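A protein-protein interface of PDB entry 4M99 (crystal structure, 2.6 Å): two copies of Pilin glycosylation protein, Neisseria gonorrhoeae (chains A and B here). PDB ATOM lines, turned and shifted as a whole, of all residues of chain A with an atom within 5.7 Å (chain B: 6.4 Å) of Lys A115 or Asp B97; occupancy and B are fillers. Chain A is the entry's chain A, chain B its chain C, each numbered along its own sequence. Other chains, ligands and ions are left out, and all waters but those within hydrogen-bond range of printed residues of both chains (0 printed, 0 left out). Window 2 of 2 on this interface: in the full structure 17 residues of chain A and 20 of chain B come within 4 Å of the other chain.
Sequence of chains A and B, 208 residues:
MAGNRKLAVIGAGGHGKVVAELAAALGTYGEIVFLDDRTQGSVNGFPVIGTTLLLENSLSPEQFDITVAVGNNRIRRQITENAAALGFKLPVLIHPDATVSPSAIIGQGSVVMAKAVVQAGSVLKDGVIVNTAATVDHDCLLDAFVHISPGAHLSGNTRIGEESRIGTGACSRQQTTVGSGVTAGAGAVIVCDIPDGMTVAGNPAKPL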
ATOM      1  N   HIS A  95      36.577   3.376 -21.911  1.00  0.00           N
ATOM      2  CA  HIS A  95      35.203   3.807 -21.626  1.00  0.00           C
ATOM      3  C   HIS A  95      35.148   4.880 -20.521  1.00  0.00           C
ATOM      4  O   HIS A  95      35.870   4.778 -19.524  1.00  0.00           O
ATOM      5  CB  HIS A  95      34.358   2.614 -21.202  1.00  0.00           C
ATOM      6  CG  HIS A  95      32.886   2.839 -21.346  1.00  0.00           C
ATOM      7  ND1 HIS A  95      32.140   3.525 -20.410  1.00  0.00           N
ATOM      8  CD2 HIS A  95      32.023   2.485 -22.331  1.00  0.00           C
ATOM      9  CE1 HIS A  95      30.881   3.580 -20.807  1.00  0.00           C
ATOM     10  NE2 HIS A  95      30.782   2.952 -21.967  1.00  0.00           N
ATOM     11  N   ASP A  97      33.242   5.189 -18.210  1.00  0.00           N
ATOM     12  CA  ASP A  97      32.931   4.582 -16.917  1.00  0.00           C
ATOM     13  C   ASP A  97      33.903   3.504 -16.524  1.00  0.00           C
ATOM     14  O   ASP A  97      33.637   2.738 -15.619  1.00  0.00           O
ATOM     15  CB  ASP A  97      31.519   4.031 -16.895  1.00  0.00           C
ATOM     16  CG  ASP A  97      30.493   5.101 -17.097  1.00  0.00           C
ATOM     17  OD1 ASP A  97      30.819   6.281 -16.842  1.00  0.00           O
ATOM     18  OD2 ASP A  97      29.362   4.777 -17.514  1.00  0.00           O
ATOM     19  N   ALA A  98      35.029   3.430 -17.216  1.00  0.00           N
ATOM     20  CA  ALA A  98      36.128   2.599 -16.751  1.00  0.00           C
ATOM     21  C   ALA A  98      37.001   3.457 -15.840  1.00  0.00           C
ATOM     22  O   ALA A  98      36.884   4.702 -15.830  1.00  0.00           O
ATOM     23  CB  ALA A  98      36.926   2.095 -17.914  1.00  0.00           C
ATOM     24  N   THR A  99      37.866   2.807 -15.067  1.00  0.00           N
ATOM     25  CA  THR A  99      38.820   3.541 -14.250  1.00  0.00           C
ATOM     26  C   THR A  99      40.194   3.002 -14.553  1.00  0.00           C
ATOM     27  O   THR A  99      40.492   1.859 -14.232  1.00  0.00           O
ATOM     28  CB  THR A  99      38.556   3.355 -12.743  1.00  0.00           C
ATOM     29  OG1 THR A  99      37.235   3.799 -12.425  1.00  0.00           O
ATOM     30  CG2 THR A  99      39.565   4.150 -11.917  1.00  0.00           C
ATOM     31  N   MET A 113      36.687  -1.623 -21.152  1.00  0.00           N
ATOM     32  CA  MET A 113      35.233  -1.503 -21.246  1.00  0.00           C
ATOM     33  C   MET A 113      34.572  -0.784 -20.066  1.00  0.00           C
ATOM     34  O   MET A 113      35.219  -0.497 -19.056  1.00  0.00           O
ATOM     35  CB  MET A 113      34.618  -2.893 -21.468  1.00  0.00           C
ATOM     36  CG  MET A 113      35.037  -3.523 -22.812  1.00  0.00           C
ATOM     37  SD  MET A 113      34.384  -2.615 -24.242  1.00  0.00           S
ATOM     38  CE  MET A 113      34.576  -3.837 -25.544  1.00  0.00           C
ATOM     39  N   ALA A 114      33.280  -0.495 -20.205  1.00  0.00           N
ATOM     40  CA  ALA A 114      32.500   0.056 -19.109  1.00  0.00           C
ATOM     41  C   ALA A 114      32.772  -0.702 -17.808  1.00  0.00           C
ATOM     42  O   ALA A 114      32.902  -1.942 -17.811  1.00  0.00           O
ATOM     43  CB  ALA A 114      31.027   0.042 -19.444  1.00  0.00           C
ATOM     44  N   LYS A 115      32.923   0.059 -16.718  1.00  0.00           N
ATOM     45  CA  LYS A 115      33.126  -0.484 -15.377  1.00  0.00           C
ATOM     46  C   LYS A 115      34.408  -1.297 -15.154  1.00  0.00           C
ATOM     47  O   LYS A 115      34.608  -1.856 -14.076  1.00  0.00           O
ATOM     48  CB  LYS A 115      31.921  -1.316 -14.953  1.00  0.00           C
ATOM     49  CG  LYS A 115      30.995  -0.621 -13.985  1.00  0.00           C
ATOM     50  CD  LYS A 115      30.466   0.690 -14.540  1.00  0.00           C
ATOM     51  CE  LYS A 115      29.273   1.126 -13.746  1.00  0.00           C
ATOM     52  NZ  LYS A 115      28.751   2.429 -14.221  1.00  0.00           N
ATOM     53  N   ALA A 116      35.281  -1.372 -16.148  1.00  0.00           N
ATOM     54  CA  ALA A 116      36.531  -2.102 -15.951  1.00  0.00           C
ATOM     55  C   ALA A 116      37.542  -1.215 -15.217  1.00  0.00           C
ATOM     56  O   ALA A 116      37.460   0.011 -15.265  1.00  0.00           O
ATOM     57  CB  ALA A 116      37.085  -2.581 -17.276  1.00  0.00           C
ATOM     58  N   VAL A 117      38.491  -1.833 -14.528  1.00  0.00           N
ATOM     59  CA  VAL A 117      39.483  -1.092 -13.751  1.00  0.00           C
ATOM     60  C   VAL A 117      40.879  -1.645 -14.006  1.00  0.00           C
ATOM     61  O   VAL A 117      41.079  -2.871 -14.022  1.00  0.00           O
ATOM     62  CB  VAL A 117      39.205  -1.179 -12.230  1.00  0.00           C
ATOM     63  CG1 VAL A 117      40.181  -0.296 -11.444  1.00  0.00           C
ATOM     64  CG2 VAL A 117      37.765  -0.816 -11.913  1.00  0.00           C
ATOM     65  N   THR A 132      33.812  -5.973 -20.079  1.00  0.00           N
ATOM     66  CA  THR A 132      32.861  -5.385 -19.125  1.00  0.00           C
ATOM     67  C   THR A 132      33.125  -5.724 -17.649  1.00  0.00           C
ATOM     68  O   THR A 132      33.101  -6.885 -17.257  1.00  0.00           O
ATOM     69  CB  THR A 132      31.417  -5.776 -19.464  1.00  0.00           C
ATOM     70  OG1 THR A 132      31.241  -5.751 -20.885  1.00  0.00           O
ATOM     71  CG2 THR A 132      30.409  -4.808 -18.807  1.00  0.00           C
ATOM     72  N   ALA A 133      33.386  -4.697 -16.838  1.00  0.00           N
ATOM     73  CA  ALA A 133      33.554  -4.862 -15.389  1.00  0.00           C
ATOM     74  C   ALA A 133      34.708  -5.799 -14.978  1.00  0.00           C
ATOM     75  O   ALA A 133      34.786  -6.246 -13.838  1.00  0.00           O
ATOM     76  CB  ALA A 133      32.240  -5.296 -14.737  1.00  0.00           C
ATOM     77  N   ALA A 134      35.609  -6.080 -15.909  1.00  0.00           N
ATOM     78  CA  ALA A 134      36.814  -6.818 -15.581  1.00  0.00           C
ATOM     79  C   ALA A 134      37.810  -5.912 -14.852  1.00  0.00           C
ATOM     80  O   ALA A 134      37.933  -4.723 -15.154  1.00  0.00           O
ATOM     81  CB  ALA A 134      37.434  -7.369 -16.835  1.00  0.00           C
ATOM     82  N   THR A 135      38.527  -6.461 -13.886  1.00  0.00           N
ATOM     83  CA  THR A 135      39.537  -5.672 -13.196  1.00  0.00           C
ATOM     84  C   THR A 135      40.929  -6.296 -13.251  1.00  0.00           C
ATOM     85  O   THR A 135      41.120  -7.482 -12.986  1.00  0.00           O
ATOM     86  CB  THR A 135      39.157  -5.392 -11.737  1.00  0.00           C
ATOM     87  OG1 THR A 135      39.072  -6.626 -11.011  1.00  0.00           O
ATOM     88  CG2 THR A 135      37.825  -4.646 -11.674  1.00  0.00           C
ATOM     89  N   ILE B  94      17.238   3.572 -13.183  1.00  0.00           N
ATOM     90  CA  ILE B  94      18.638   3.253 -13.453  1.00  0.00           C
ATOM     91  C   ILE B  94      19.573   4.047 -12.557  1.00  0.00           C
ATOM     92  O   ILE B  94      19.607   5.272 -12.608  1.00  0.00           O
ATOM     93  CB  ILE B  94      18.992   3.471 -14.933  1.00  0.00           C
ATOM     94  CG1 ILE B  94      18.094   2.588 -15.815  1.00  0.00           C
ATOM     95  CG2 ILE B  94      20.492   3.191 -15.175  1.00  0.00           C
ATOM     96  CD1 ILE B  94      18.347   2.698 -17.296  1.00  0.00           C
ATOM     97  N   HIS B  95      20.310   3.343 -11.711  1.00  0.00           N
ATOM     98  CA  HIS B  95      21.205   4.007 -10.786  1.00  0.00           C
ATOM     99  C   HIS B  95      22.205   4.848 -11.567  1.00  0.00           C
ATOM    100  O   HIS B  95      22.705   4.406 -12.612  1.00  0.00           O
ATOM    101  CB  HIS B  95      21.958   2.991  -9.933  1.00  0.00           C
ATOM    102  CG  HIS B  95      22.582   3.588  -8.707  1.00  0.00           C
ATOM    103  ND1 HIS B  95      23.824   4.186  -8.717  1.00  0.00           N
ATOM    104  CD2 HIS B  95      22.121   3.699  -7.438  1.00  0.00           C
ATOM    105  CE1 HIS B  95      24.109   4.629  -7.505  1.00  0.00           C
ATOM    106  NE2 HIS B  95      23.094   4.343  -6.710  1.00  0.00           N
ATOM    107  N   PRO B  96      22.502   6.056 -11.065  1.00  0.00           N
ATOM    108  CA  PRO B  96      23.448   6.936 -11.757  1.00  0.00           C
ATOM    109  C   PRO B  96      24.778   6.255 -12.007  1.00  0.00           C
ATOM    110  O   PRO B  96      25.416   6.522 -13.020  1.00  0.00           O
ATOM    111  CB  PRO B  96      23.603   8.122 -10.790  1.00  0.00           C
ATOM    112  CG  PRO B  96      22.283   8.188 -10.070  1.00  0.00           C
ATOM    113  CD  PRO B  96      21.881   6.716  -9.901  1.00  0.00           C
ATOM    114  N   ASP B  97      25.177   5.358 -11.117  1.00  0.00           N
ATOM    115  CA  ASP B  97      26.452   4.675 -11.280  1.00  0.00           C
ATOM    116  C   ASP B  97      26.307   3.358 -12.021  1.00  0.00           C
ATOM    117  O   ASP B  97      27.204   2.520 -12.005  1.00  0.00           O
ATOM    118  CB  ASP B  97      27.156   4.484  -9.933  1.00  0.00           C
ATOM    119  CG  ASP B  97      27.486   5.801  -9.263  1.00  0.00           C
ATOM    120  OD1 ASP B  97      27.602   6.816  -9.983  1.00  0.00           O
ATOM    121  OD2 ASP B  97      27.612   5.833  -8.018  1.00  0.00           O
ATOM    122  N   ALA B  98      25.172   3.170 -12.679  1.00  0.00           N
ATOM    123  CA  ALA B  98      25.069   2.068 -13.624  1.00  0.00           C
ATOM    124  C   ALA B  98      25.367   2.617 -15.009  1.00  0.00           C
ATOM    125  O   ALA B  98      25.147   3.802 -15.280  1.00  0.00           O
ATOM    126  CB  ALA B  98      23.681   1.425 -13.581  1.00  0.00           C
ATOM    127  N   THR B  99      25.884   1.762 -15.881  1.00  0.00           N
ATOM    128  CA  THR B  99      26.009   2.097 -17.286  1.00  0.00           C
ATOM    129  C   THR B  99      25.031   1.267 -18.118  1.00  0.00           C
ATOM    130  O   THR B  99      25.183   0.049 -18.234  1.00  0.00           O
ATOM    131  CB  THR B  99      27.403   1.797 -17.767  1.00  0.00           C
ATOM    132  OG1 THR B  99      28.339   2.338 -16.830  1.00  0.00           O
ATOM    133  CG2 THR B  99      27.618   2.405 -19.135  1.00  0.00           C
ATOM    134  N   MET B 113      20.863  -1.513 -10.696  1.00  0.00           N
ATOM    135  CA  MET B 113      21.555  -1.047  -9.492  1.00  0.00           C
ATOM    136  C   MET B 113      22.900  -0.402  -9.784  1.00  0.00           C
ATOM    137  O   MET B 113      23.432  -0.523 -10.893  1.00  0.00           O
ATOM    138  CB  MET B 113      21.778  -2.215  -8.519  1.00  0.00           C
ATOM    139  CG  MET B 113      20.515  -2.823  -7.955  1.00  0.00           C
ATOM    140  SD  MET B 113      19.471  -1.616  -7.098  1.00  0.00           S
ATOM    141  CE  MET B 113      18.376  -2.735  -6.218  1.00  0.00           C
ATOM    142  N   ALA B 114      23.443   0.282  -8.775  1.00  0.00           N
ATOM    143  CA  ALA B 114      24.792   0.834  -8.843  1.00  0.00           C
ATOM    144  C   ALA B 114      25.803  -0.173  -9.411  1.00  0.00           C
ATOM    145  O   ALA B 114      25.708  -1.379  -9.167  1.00  0.00           O
ATOM    146  CB  ALA B 114      25.226   1.316  -7.474  1.00  0.00           C
ATOM    147  N   LYS B 115      26.741   0.342 -10.201  1.00  0.00           N
ATOM    148  CA  LYS B 115      27.770  -0.457 -10.873  1.00  0.00           C
ATOM    149  C   LYS B 115      27.272  -1.530 -11.844  1.00  0.00           C
ATOM    150  O   LYS B 115      28.086  -2.250 -12.438  1.00  0.00           O
ATOM    151  CB  LYS B 115      28.766  -1.056  -9.872  1.00  0.00           C
ATOM    152  CG  LYS B 115      30.047  -0.245  -9.725  1.00  0.00           C
ATOM    153  CD  LYS B 115      29.765   1.213  -9.363  1.00  0.00           C
ATOM    154  CE  LYS B 115      31.067   1.967  -9.077  1.00  0.00           C
ATOM    155  NZ  LYS B 115      30.864   3.382  -8.630  1.00  0.00           N
ATOM    156  N   ALA B 116      25.960  -1.652 -12.024  1.00  0.00           N
ATOM    157  CA  ALA B 116      25.462  -2.643 -12.988  1.00  0.00           C
ATOM    158  C   ALA B 116      25.724  -2.145 -14.407  1.00  0.00           C
ATOM    159  O   ALA B 116      25.836  -0.934 -14.638  1.00  0.00           O
ATOM    160  CB  ALA B 116      23.975  -2.936 -12.786  1.00  0.00           C
ATOM    161  N   VAL B 117      25.835  -3.069 -15.352  1.00  0.00           N
ATOM    162  CA  VAL B 117      26.019  -2.693 -16.749  1.00  0.00           C
ATOM    163  C   VAL B 117      25.134  -3.526 -17.653  1.00  0.00           C
ATOM    164  O   VAL B 117      25.102  -4.754 -17.550  1.00  0.00           O
ATOM    165  CB  VAL B 117      27.459  -2.930 -17.246  1.00  0.00           C
ATOM    166  CG1 VAL B 117      27.637  -2.330 -18.643  1.00  0.00           C
ATOM    167  CG2 VAL B 117      28.480  -2.376 -16.282  1.00  0.00           C
ATOM    168  N   THR B 135      26.495  -7.658 -14.469  1.00  0.00           N
ATOM    169  CA  THR B 135      26.611  -7.197 -15.833  1.00  0.00           C
ATOM    170  C   THR B 135      25.912  -8.121 -16.836  1.00  0.00           C
ATOM    171  O   THR B 135      26.001  -9.348 -16.761  1.00  0.00           O
ATOM    172  CB  THR B 135      28.071  -6.961 -16.222  1.00  0.00           C
ATOM    173  OG1 THR B 135      28.790  -8.200 -16.182  1.00  0.00           O
ATOM    174  CG2 THR B 135      28.707  -5.967 -15.262  1.00  0.00           C
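NZ of Lys A115 lies within hydrogen-bond range of OG1 of Thr B99 (2.6 Å). NZ of Lys A115 is in hydrogen-bond range of O of Asp B97, at 2.7 Å. The side-chain hydroxyl of Thr B99 lies within hydrogen-bond range of the side-chain carboxylate of Asp A97.
The backbone NH (N) of Ala A133 sits at hydrogen-bond distance from the backbone carbonyl oxygen (O) of Ala A114 (3.0 Å). The backbone NH (N) of Asp B97 sits at hydrogen-bond distance from a ring nitrogen (ND1) of His B95 (3.0 Å). The backbone carbonyl oxygen (O) of Asp B97 sits at hydrogen-bond distance from the backbone NH (N) of Lys B115, 2.9 Å away. N of Thr B99 lies within hydrogen-bond range of O of Ala B116 (3.0 Å). O of Asp A97 is in hydrogen-bond range of N of Lys A115 (3.0 Å). The backbone NH (N) of Asp A97 lies within hydrogen-bond range of a ring nitrogen (ND1) of His A95 (3.0 Å).
CG2 of Thr B99 touches CE1 of His A95, 3.9 Å away. Ala B98 touches Lys A115. CA of Lys B115 touches CE of Lys A115, 3.6 Å away. Val B117 touches Lys A115 (CG2 to CG, 3.8 Å). Thr A132 touches Val B117 (CG2 to CG1, 3.7 Å). CB of Ala A133 touches CG2 of Thr B135 (3.6 Å).
Of chain B, only Asp B97, Ala B98, Thr B99, Lys B115 and Val B117 come within 4 Å of Lys A115. Printed residues of chain A within 4 Å of Asp B97: Lys A115 (2.7 Å). Of the printed residues of chain A, Thr B135 touches Ala A133 (3.6 Å). Of the printed residues of chain A, Val B117 touches Lys A115 (3.8 Å) and Thr A132 (3.7 Å). Thr A99 touches none of the printed residues of chain B. Val A117 touches none of the printed residues of chain B. The nearest printed residue of chain A that does not touch Asp B97 is Asp A97 (6.3 Å).
Of the 13 printed residues of chain A, 5 touch a printed residue of chain B. Hydrophobic or aromatic side chains of chain A that line the printed part of chain B: His A95 and Ala A133.
Asp A97 touches Thr B99, but with the chains exchanged Thr A99 does not touch Asp B97 (10.1 Å). Lys A115 touches Asp B97, but with the chains exchanged Asp A97 does not touch Lys B115 (7.1 Å). Lys A115 touches Ala B98, but with the chains exchanged Ala A98 does not touch Lys B115 (9.1 Å). Lys A115 touches Thr B99, but with the chains exchanged Thr A99 does not touch Lys B115 (7.3 Å). Positions printed for both chains: 95, 97, 98, 99, 113, 114, 115, 116, 117 and 135. Of the 9 pairs that touch across the chains among the printed residues, 1 has its exchanged pair printed and touching as well.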
